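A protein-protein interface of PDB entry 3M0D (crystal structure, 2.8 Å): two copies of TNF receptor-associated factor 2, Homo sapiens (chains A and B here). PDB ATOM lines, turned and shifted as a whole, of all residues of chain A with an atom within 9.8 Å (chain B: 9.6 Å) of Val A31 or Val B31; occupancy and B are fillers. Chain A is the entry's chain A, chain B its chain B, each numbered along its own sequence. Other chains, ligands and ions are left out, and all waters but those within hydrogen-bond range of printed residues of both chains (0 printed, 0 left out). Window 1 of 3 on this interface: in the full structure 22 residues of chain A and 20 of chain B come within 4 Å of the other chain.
Among the printed residues, pairs that only touch across the chains: Leu A24 with Leu B24, Asn A25 with Leu B24, Asn A25 with Glu B27, Val A28 with Val B28, Val A28 with Val B31, Val A31 with Val B31 and Ala A35 with Thr B34.
SG of Cys B38 lies within hydrogen-bond range of O of Ala A35 (3.8 Å).
The side-chain hydroxyl (OG) of Ser A39 is in hydrogen-bond range of the side-chain sulfur (SG) of Cys B38 (3.6 Å).
Leu A24 touches its own counterpart, Leu B24.
Asn A25 touches Glu B27, but with the chains exchanged Glu A27 does not touch Asn B25 (12.2 Å).
Val A31 touches its own counterpart, Val B31.
Ala A35 touches Thr B34, but with the chains exchanged Thr A34 does not touch Ala B35 (7.7 Å).
17 positions are printed for both chains.
Of the 9 pairs that touch across the chains among the printed residues, 3 have their exchanged pair printed and touching as well.
The backbone carbonyl oxygen (O) of Thr B34 is in hydrogen-bond range of the side-chain sulfur (SG) of Cys B38, at 3.5 Å.
The backbone carbonyl oxygen of Arg B30 sits at hydrogen-bond distance from the side-chain hydroxyl of Thr B34, at 3.3 Å.
Of chain B, only Val B31 (3.1 Å) comes within 4 Å of Val A31.
Val B31 touches two residues of chain A.
Of chain B, only Val B28 (3.98 Å) and Val B31 (3.7 Å) come within 4 Å of Val A28.
No residue of chain B comes within 4 Å of Thr A34.
Of the printed residues of chain A, Thr B34 touches Ala A35.
Of the printed residues of chain A, Glu B27 touches Asn A25.
Of the printed residues of chain A, Cys B38 touches Ala A35 (3.8 Å) and Ser A39 (3.6 Å).
Val A23 touches none of the printed residues of chain B.
The nearest residue of chain B that does not touch Val A31 is Ala B35 (4.9 Å).
The nearest printed residue of chain A that does not touch Leu B24 is Val A28 (4.8 Å).
Of the 17 printed residues of chain A, 6 touch a printed residue of chain B.
Hydrophobic or aromatic side chains of chain A that line the printed part of chain B: Leu A24, Val A28, Val A31 and Ala A35.
Of the 17 printed residues of chain B, 6 touch a printed residue of chain A.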
ATOM      1  N   VAL A  23      14.994  22.217 -19.420  1.00  0.00           N
ATOM      2  CA  VAL A  23      14.751  21.848 -20.807  1.00  0.00           C
ATOM      3  C   VAL A  23      15.636  22.626 -21.779  1.00  0.00           C
ATOM      4  O   VAL A  23      16.173  22.071 -22.750  1.00  0.00           O
ATOM      5  CB  VAL A  23      13.268  22.112 -21.215  1.00  0.00           C
ATOM      6  CG1 VAL A  23      13.047  21.777 -22.688  1.00  0.00           C
ATOM      7  CG2 VAL A  23      12.311  21.316 -20.361  1.00  0.00           C
ATOM      8  N   LEU A  24      15.758  23.925 -21.536  1.00  0.00           N
ATOM      9  CA  LEU A  24      16.614  24.748 -22.373  1.00  0.00           C
ATOM     10  C   LEU A  24      18.009  24.162 -22.421  1.00  0.00           C
ATOM     11  O   LEU A  24      18.561  23.979 -23.505  1.00  0.00           O
ATOM     12  CB  LEU A  24      16.674  26.172 -21.855  1.00  0.00           C
ATOM     13  CG  LEU A  24      17.589  27.081 -22.655  1.00  0.00           C
ATOM     14  CD1 LEU A  24      17.225  27.035 -24.141  1.00  0.00           C
ATOM     15  CD2 LEU A  24      17.521  28.496 -22.100  1.00  0.00           C
ATOM     16  N   ASN A  25      18.577  23.861 -21.262  1.00  0.00           N
ATOM     17  CA  ASN A  25      19.902  23.275 -21.217  1.00  0.00           C
ATOM     18  C   ASN A  25      20.020  21.994 -22.022  1.00  0.00           C
ATOM     19  O   ASN A  25      21.011  21.779 -22.729  1.00  0.00           O
ATOM     20  CB  ASN A  25      20.322  22.987 -19.781  1.00  0.00           C
ATOM     21  CG  ASN A  25      20.971  24.164 -19.120  1.00  0.00           C
ATOM     22  OD1 ASN A  25      20.672  24.473 -17.977  1.00  0.00           O
ATOM     23  ND2 ASN A  25      21.835  24.851 -19.839  1.00  0.00           N
ATOM     24  N   ARG A  26      19.021  21.132 -21.887  1.00  0.00           N
ATOM     25  CA  ARG A  26      19.021  19.876 -22.615  1.00  0.00           C
ATOM     26  C   ARG A  26      19.109  20.176 -24.114  1.00  0.00           C
ATOM     27  O   ARG A  26      19.898  19.563 -24.818  1.00  0.00           O
ATOM     28  CB  ARG A  26      17.786  19.026 -22.267  1.00  0.00           C
ATOM     29  CG  ARG A  26      17.805  17.578 -22.776  1.00  0.00           C
ATOM     30  CD  ARG A  26      18.999  16.783 -22.244  1.00  0.00           C
ATOM     31  NE  ARG A  26      19.205  15.486 -22.911  1.00  0.00           N
ATOM     32  CZ  ARG A  26      19.788  15.332 -24.109  1.00  0.00           C
ATOM     33  NH1 ARG A  26      20.209  16.380 -24.809  1.00  0.00           N
ATOM     34  NH2 ARG A  26      19.939  14.124 -24.620  1.00  0.00           N
ATOM     35  N   GLU A  27      18.324  21.138 -24.599  1.00  0.00           N
ATOM     36  CA  GLU A  27      18.296  21.425 -26.037  1.00  0.00           C
ATOM     37  C   GLU A  27      19.583  22.043 -26.548  1.00  0.00           C
ATOM     38  O   GLU A  27      20.050  21.695 -27.629  1.00  0.00           O
ATOM     39  CB  GLU A  27      17.092  22.276 -26.432  1.00  0.00           C
ATOM     40  CG  GLU A  27      15.738  21.579 -26.227  1.00  0.00           C
ATOM     41  CD  GLU A  27      15.631  20.205 -26.899  1.00  0.00           C
ATOM     42  OE1 GLU A  27      16.145  20.032 -28.034  1.00  0.00           O
ATOM     43  OE2 GLU A  27      15.027  19.297 -26.277  1.00  0.00           O
ATOM     44  N   VAL A  28      20.174  22.942 -25.769  1.00  0.00           N
ATOM     45  CA  VAL A  28      21.504  23.440 -26.100  1.00  0.00           C
ATOM     46  C   VAL A  28      22.447  22.264 -26.342  1.00  0.00           C
ATOM     47  O   VAL A  28      23.179  22.236 -27.331  1.00  0.00           O
ATOM     48  CB  VAL A  28      22.066  24.335 -24.989  1.00  0.00           C
ATOM     49  CG1 VAL A  28      23.512  24.705 -25.280  1.00  0.00           C
ATOM     50  CG2 VAL A  28      21.238  25.584 -24.880  1.00  0.00           C
ATOM     51  N   GLU A  29      22.406  21.284 -25.445  1.00  0.00           N
ATOM     52  CA  GLU A  29      23.229  20.087 -25.582  1.00  0.00           C
ATOM     53  C   GLU A  29      22.934  19.299 -26.864  1.00  0.00           C
ATOM     54  O   GLU A  29      23.865  18.815 -27.518  1.00  0.00           O
ATOM     55  CB  GLU A  29      23.096  19.190 -24.348  1.00  0.00           C
ATOM     56  CG  GLU A  29      23.699  17.805 -24.490  1.00  0.00           C
ATOM     57  CD  GLU A  29      25.225  17.803 -24.515  1.00  0.00           C
ATOM     58  OE1 GLU A  29      25.828  18.811 -24.054  1.00  0.00           O
ATOM     59  OE2 GLU A  29      25.806  16.785 -24.991  1.00  0.00           O
ATOM     60  N   ARG A  30      21.657  19.152 -27.217  1.00  0.00           N
ATOM     61  CA  ARG A  30      21.319  18.439 -28.435  1.00  0.00           C
ATOM     62  C   ARG A  30      21.768  19.245 -29.683  1.00  0.00           C
ATOM     63  O   ARG A  30      22.239  18.670 -30.679  1.00  0.00           O
ATOM     64  CB  ARG A  30      19.822  18.047 -28.484  1.00  0.00           C
ATOM     65  CG  ARG A  30      19.435  17.114 -29.683  1.00  0.00           C
ATOM     66  CD  ARG A  30      18.204  16.183 -29.431  1.00  0.00           C
ATOM     67  NE  ARG A  30      18.529  14.897 -28.789  1.00  0.00           N
ATOM     68  CZ  ARG A  30      17.631  13.958 -28.464  1.00  0.00           C
ATOM     69  NH1 ARG A  30      16.338  14.141 -28.718  1.00  0.00           N
ATOM     70  NH2 ARG A  30      18.016  12.826 -27.874  1.00  0.00           N
ATOM     71  N   VAL A  31      21.644  20.571 -29.621  1.00  0.00           N
ATOM     72  CA  VAL A  31      22.112  21.415 -30.720  1.00  0.00           C
ATOM     73  C   VAL A  31      23.641  21.344 -30.832  1.00  0.00           C
ATOM     74  O   VAL A  31      24.192  21.205 -31.928  1.00  0.00           O
ATOM     75  CB  VAL A  31      21.646  22.894 -30.589  1.00  0.00           C
ATOM     76  CG1 VAL A  31      22.427  23.790 -31.538  1.00  0.00           C
ATOM     77  CG2 VAL A  31      20.144  23.032 -30.857  1.00  0.00           C
ATOM     78  N   ALA A  32      24.317  21.423 -29.691  1.00  0.00           N
ATOM     79  CA  ALA A  32      25.761  21.321 -29.663  1.00  0.00           C
ATOM     80  C   ALA A  32      26.220  20.002 -30.288  1.00  0.00           C
ATOM     81  O   ALA A  32      27.225  19.968 -31.009  1.00  0.00           O
ATOM     82  CB  ALA A  32      26.276  21.459 -28.235  1.00  0.00           C
ATOM     83  N   MET A  33      25.483  18.926 -30.015  1.00  0.00           N
ATOM     84  CA  MET A  33      25.841  17.595 -30.509  1.00  0.00           C
ATOM     85  C   MET A  33      25.587  17.413 -31.997  1.00  0.00           C
ATOM     86  O   MET A  33      26.399  16.801 -32.709  1.00  0.00           O
ATOM     87  CB  MET A  33      25.118  16.494 -29.733  1.00  0.00           C
ATOM     88  CG  MET A  33      25.709  16.218 -28.355  1.00  0.00           C
ATOM     89  SD  MET A  33      27.482  15.854 -28.365  1.00  0.00           S
ATOM     90  CE  MET A  33      28.145  17.358 -27.613  1.00  0.00           C
ATOM     91  N   THR A  34      24.458  17.928 -32.468  1.00  0.00           N
ATOM     92  CA  THR A  34      24.134  17.797 -33.884  1.00  0.00           C
ATOM     93  C   THR A  34      24.921  18.794 -34.740  1.00  0.00           C
ATOM     94  O   THR A  34      24.997  18.633 -35.953  1.00  0.00           O
ATOM     95  CB  THR A  34      22.608  17.839 -34.178  1.00  0.00           C
ATOM     96  OG1 THR A  34      22.075  19.105 -33.820  1.00  0.00           O
ATOM     97  CG2 THR A  34      21.865  16.747 -33.395  1.00  0.00           C
ATOM     98  N   ALA A  35      25.525  19.802 -34.111  1.00  0.00           N
ATOM     99  CA  ALA A  35      26.524  20.636 -34.809  1.00  0.00           C
ATOM    100  C   ALA A  35      27.906  19.947 -34.918  1.00  0.00           C
ATOM    101  O   ALA A  35      28.576  20.050 -35.953  1.00  0.00           O
ATOM    102  CB  ALA A  35      26.651  22.038 -34.174  1.00  0.00           C
ATOM    103  N   GLU A  36      28.317  19.251 -33.853  1.00  0.00           N
ATOM    104  CA  GLU A  36      29.519  18.427 -33.896  1.00  0.00           C
ATOM    105  C   GLU A  36      29.390  17.402 -35.021  1.00  0.00           C
ATOM    106  O   GLU A  36      30.319  17.195 -35.792  1.00  0.00           O
ATOM    107  CB  GLU A  36      29.752  17.711 -32.561  1.00  0.00           C
ATOM    108  N   ALA A  37      28.222  16.778 -35.127  1.00  0.00           N
ATOM    109  CA  ALA A  37      27.994  15.763 -36.147  1.00  0.00           C
ATOM    110  C   ALA A  37      27.909  16.371 -37.542  1.00  0.00           C
ATOM    111  O   ALA A  37      28.450  15.818 -38.514  1.00  0.00           O
ATOM    112  CB  ALA A  37      26.743  15.000 -35.842  1.00  0.00           C
ATOM    113  N   CYS A  38      27.210  17.498 -37.646  1.00  0.00           N
ATOM    114  CA  CYS A  38      27.110  18.184 -38.919  1.00  0.00           C
ATOM    115  C   CYS A  38      28.524  18.428 -39.454  1.00  0.00           C
ATOM    116  O   CYS A  38      28.810  18.155 -40.630  1.00  0.00           O
ATOM    117  CB  CYS A  38      26.340  19.494 -38.765  1.00  0.00           C
ATOM    118  SG  CYS A  38      26.209  20.504 -40.252  1.00  0.00           S
ATOM    119  N   SER A  39      29.403  18.908 -38.571  1.00  0.00           N
ATOM    120  CA  SER A  39      30.799  19.206 -38.913  1.00  0.00           C
ATOM    121  C   SER A  39      31.733  17.993 -39.063  1.00  0.00           C
ATOM    122  O   SER A  39      32.815  18.104 -39.645  1.00  0.00           O
ATOM    123  CB  SER A  39      31.398  20.219 -37.932  1.00  0.00           C
ATOM    124  OG  SER A  39      31.177  21.536 -38.400  1.00  0.00           O
ATOM    125  N   VAL B  23      25.429  32.470 -17.525  1.00  0.00           N
ATOM    126  CA  VAL B  23      26.067  31.377 -18.230  1.00  0.00           C
ATOM    127  C   VAL B  23      25.291  30.905 -19.472  1.00  0.00           C
ATOM    128  O   VAL B  23      25.870  30.782 -20.556  1.00  0.00           O
ATOM    129  CB  VAL B  23      26.279  30.197 -17.297  1.00  0.00           C
ATOM    130  CG1 VAL B  23      26.640  28.967 -18.102  1.00  0.00           C
ATOM    131  CG2 VAL B  23      27.357  30.521 -16.287  1.00  0.00           C
ATOM    132  N   LEU B  24      24.000  30.625 -19.308  1.00  0.00           N
ATOM    133  CA  LEU B  24      23.142  30.195 -20.414  1.00  0.00           C
ATOM    134  C   LEU B  24      23.220  31.166 -21.564  1.00  0.00           C
ATOM    135  O   LEU B  24      23.264  30.773 -22.733  1.00  0.00           O
ATOM    136  CB  LEU B  24      21.685  30.128 -19.969  1.00  0.00           C
ATOM    137  CG  LEU B  24      21.202  28.792 -19.433  1.00  0.00           C
ATOM    138  CD1 LEU B  24      19.915  28.995 -18.670  1.00  0.00           C
ATOM    139  CD2 LEU B  24      21.031  27.774 -20.565  1.00  0.00           C
ATOM    140  N   ASN B  25      23.206  32.451 -21.231  1.00  0.00           N
ATOM    141  CA  ASN B  25      23.302  33.466 -22.252  1.00  0.00           C
ATOM    142  C   ASN B  25      24.585  33.321 -23.093  1.00  0.00           C
ATOM    143  O   ASN B  25      24.550  33.433 -24.323  1.00  0.00           O
ATOM    144  CB  ASN B  25      23.209  34.839 -21.629  1.00  0.00           C
ATOM    145  CG  ASN B  25      23.225  35.928 -22.659  1.00  0.00           C
ATOM    146  OD1 ASN B  25      22.568  35.819 -23.678  1.00  0.00           O
ATOM    147  ND2 ASN B  25      24.003  36.973 -22.420  1.00  0.00           N
ATOM    148  N   ARG B  26      25.709  33.057 -22.429  1.00  0.00           N
ATOM    149  CA  ARG B  26      26.935  32.743 -23.142  1.00  0.00           C
ATOM    150  C   ARG B  26      26.790  31.470 -23.973  1.00  0.00           C
ATOM    151  O   ARG B  26      27.070  31.462 -25.178  1.00  0.00           O
ATOM    152  CB  ARG B  26      28.094  32.592 -22.172  1.00  0.00           C
ATOM    153  CG  ARG B  26      28.702  33.899 -21.765  1.00  0.00           C
ATOM    154  CD  ARG B  26      29.940  33.684 -20.925  1.00  0.00           C
ATOM    155  NE  ARG B  26      30.132  34.814 -20.022  1.00  0.00           N
ATOM    156  CZ  ARG B  26      29.907  34.775 -18.711  1.00  0.00           C
ATOM    157  NH1 ARG B  26      29.504  33.649 -18.129  1.00  0.00           N
ATOM    158  NH2 ARG B  26      30.103  35.862 -17.978  1.00  0.00           N
ATOM    159  N   GLU B  27      26.353  30.393 -23.331  1.00  0.00           N
ATOM    160  CA  GLU B  27      26.250  29.115 -24.022  1.00  0.00           C
ATOM    161  C   GLU B  27      25.313  29.148 -25.236  1.00  0.00           C
ATOM    162  O   GLU B  27      25.631  28.588 -26.282  1.00  0.00           O
ATOM    163  CB  GLU B  27      25.877  28.019 -23.036  1.00  0.00           C
ATOM    164  CG  GLU B  27      26.853  27.965 -21.871  1.00  0.00           C
ATOM    165  CD  GLU B  27      26.464  26.950 -20.812  1.00  0.00           C
ATOM    166  OE1 GLU B  27      25.359  26.368 -20.920  1.00  0.00           O
ATOM    167  OE2 GLU B  27      27.265  26.734 -19.874  1.00  0.00           O
ATOM    168  N   VAL B  28      24.179  29.830 -25.115  1.00  0.00           N
ATOM    169  CA  VAL B  28      23.243  29.949 -26.234  1.00  0.00           C
ATOM    170  C   VAL B  28      23.819  30.794 -27.372  1.00  0.00           C
ATOM    171  O   VAL B  28      23.721  30.418 -28.538  1.00  0.00           O
ATOM    172  CB  VAL B  28      21.875  30.522 -25.784  1.00  0.00           C
ATOM    173  CG1 VAL B  28      20.991  30.801 -26.977  1.00  0.00           C
ATOM    174  CG2 VAL B  28      21.188  29.562 -24.837  1.00  0.00           C
ATOM    175  N   GLU B  29      24.415  31.933 -27.038  1.00  0.00           N
ATOM    176  CA  GLU B  29      25.139  32.722 -28.034  1.00  0.00           C
ATOM    177  C   GLU B  29      26.204  31.877 -28.774  1.00  0.00           C
ATOM    178  O   GLU B  29      26.302  31.903 -30.007  1.00  0.00           O
ATOM    179  CB  GLU B  29      25.812  33.909 -27.352  1.00  0.00           C
ATOM    180  CG  GLU B  29      26.173  35.077 -28.263  1.00  0.00           C
ATOM    181  CD  GLU B  29      26.820  36.255 -27.521  1.00  0.00           C
ATOM    182  OE1 GLU B  29      27.037  37.309 -28.166  1.00  0.00           O
ATOM    183  OE2 GLU B  29      27.112  36.136 -26.304  1.00  0.00           O
ATOM    184  N   ARG B  30      26.992  31.130 -28.004  1.00  0.00           N
ATOM    185  CA  ARG B  30      28.075  30.325 -28.543  1.00  0.00           C
ATOM    186  C   ARG B  30      27.531  29.257 -29.485  1.00  0.00           C
ATOM    187  O   ARG B  30      28.048  29.056 -30.575  1.00  0.00           O
ATOM    188  CB  ARG B  30      28.862  29.662 -27.410  1.00  0.00           C
ATOM    189  CG  ARG B  30      30.281  29.251 -27.790  1.00  0.00           C
ATOM    190  CD  ARG B  30      30.892  28.214 -26.833  1.00  0.00           C
ATOM    191  NE  ARG B  30      30.127  28.059 -25.590  1.00  0.00           N
ATOM    192  CZ  ARG B  30      30.489  28.529 -24.394  1.00  0.00           C
ATOM    193  NH1 ARG B  30      31.627  29.202 -24.247  1.00  0.00           N
ATOM    194  NH2 ARG B  30      29.706  28.318 -23.341  1.00  0.00           N
ATOM    195  N   VAL B  31      26.487  28.566 -29.052  1.00  0.00           N
ATOM    196  CA  VAL B  31      25.884  27.519 -29.863  1.00  0.00           C
ATOM    197  C   VAL B  31      25.269  28.071 -31.147  1.00  0.00           C
ATOM    198  O   VAL B  31      25.488  27.511 -32.218  1.00  0.00           O
ATOM    199  CB  VAL B  31      24.836  26.728 -29.057  1.00  0.00           C
ATOM    200  CG1 VAL B  31      23.879  26.074 -29.974  1.00  0.00           C
ATOM    201  CG2 VAL B  31      25.516  25.677 -28.198  1.00  0.00           C
ATOM    202  N   ALA B  32      24.508  29.162 -31.032  1.00  0.00           N
ATOM    203  CA  ALA B  32      23.971  29.867 -32.196  1.00  0.00           C
ATOM    204  C   ALA B  32      25.076  30.137 -33.227  1.00  0.00           C
ATOM    205  O   ALA B  32      24.909  29.912 -34.434  1.00  0.00           O
ATOM    206  CB  ALA B  32      23.347  31.166 -31.772  1.00  0.00           C
ATOM    207  N   MET B  33      26.180  30.668 -32.707  1.00  0.00           N
ATOM    208  CA  MET B  33      27.416  30.928 -33.416  1.00  0.00           C
ATOM    209  C   MET B  33      27.871  29.719 -34.232  1.00  0.00           C
ATOM    210  O   MET B  33      28.149  29.820 -35.427  1.00  0.00           O
ATOM    211  CB  MET B  33      28.490  31.217 -32.365  1.00  0.00           C
ATOM    212  CG  MET B  33      29.539  32.248 -32.731  1.00  0.00           C
ATOM    213  SD  MET B  33      28.885  33.917 -32.660  1.00  0.00           S
ATOM    214  CE  MET B  33      27.866  33.969 -34.152  1.00  0.00           C
ATOM    215  N   THR B  34      27.975  28.588 -33.545  1.00  0.00           N
ATOM    216  CA  THR B  34      28.445  27.344 -34.112  1.00  0.00           C
ATOM    217  C   THR B  34      27.560  26.907 -35.244  1.00  0.00           C
ATOM    218  O   THR B  34      28.040  26.612 -36.347  1.00  0.00           O
ATOM    219  CB  THR B  34      28.396  26.233 -33.066  1.00  0.00           C
ATOM    220  OG1 THR B  34      29.436  26.436 -32.100  1.00  0.00           O
ATOM    221  CG2 THR B  34      28.593  24.887 -33.729  1.00  0.00           C
ATOM    222  N   ALA B  35      26.263  26.846 -34.956  1.00  0.00           N
ATOM    223  CA  ALA B  35      25.278  26.444 -35.948  1.00  0.00           C
ATOM    224  C   ALA B  35      25.375  27.352 -37.167  1.00  0.00           C
ATOM    225  O   ALA B  35      25.404  26.878 -38.301  1.00  0.00           O
ATOM    226  CB  ALA B  35      23.882  26.476 -35.359  1.00  0.00           C
ATOM    227  N   GLU B  36      25.429  28.660 -36.932  1.00  0.00           N
ATOM    228  CA  GLU B  36      25.646  29.596 -38.025  1.00  0.00           C
ATOM    229  C   GLU B  36      26.860  29.173 -38.884  1.00  0.00           C
ATOM    230  O   GLU B  36      26.763  29.050 -40.111  1.00  0.00           O
ATOM    231  CB  GLU B  36      25.813  31.021 -37.505  1.00  0.00           C
ATOM    232  CG  GLU B  36      24.927  32.009 -38.230  1.00  0.00           C
ATOM    233  CD  GLU B  36      24.847  31.732 -39.730  1.00  0.00           C
ATOM    234  OE1 GLU B  36      25.807  32.067 -40.459  1.00  0.00           O
ATOM    235  OE2 GLU B  36      23.824  31.170 -40.188  1.00  0.00           O
ATOM    236  N   ALA B  37      27.992  28.932 -38.227  1.00  0.00           N
ATOM    237  CA  ALA B  37      29.220  28.559 -38.920  1.00  0.00           C
ATOM    238  C   ALA B  37      29.099  27.199 -39.601  1.00  0.00           C
ATOM    239  O   ALA B  37      29.870  26.876 -40.514  1.00  0.00           O
ATOM    240  CB  ALA B  37      30.387  28.567 -37.965  1.00  0.00           C
ATOM    241  N   CYS B  38      28.138  26.403 -39.150  1.00  0.00           N
ATOM    242  CA  CYS B  38      27.870  25.142 -39.812  1.00  0.00           C
ATOM    243  C   CYS B  38      27.162  25.395 -41.132  1.00  0.00           C
ATOM    244  O   CYS B  38      27.585  24.891 -42.175  1.00  0.00           O
ATOM    245  CB  CYS B  38      27.067  24.225 -38.907  1.00  0.00           C
ATOM    246  SG  CYS B  38      28.111  23.385 -37.707  1.00  0.00           S
ATOM    247  N   SER B  39      26.105  26.203 -41.082  1.00  0.00           N
ATOM    248  CA  SER B  39      25.392  26.602 -42.287  1.00  0.00           C
ATOM    249  C   SER B  39      26.346  27.198 -43.309  1.00  0.00           C
ATOM    250  O   SER B  39      26.338  26.813 -44.471  1.00  0.00           O
ATOM    251  CB  SER B  39      24.301  27.622 -41.960  1.00  0.00           C
ATOM    252  OG  SER B  39      23.303  27.039 -41.149  1.00  0.00           O
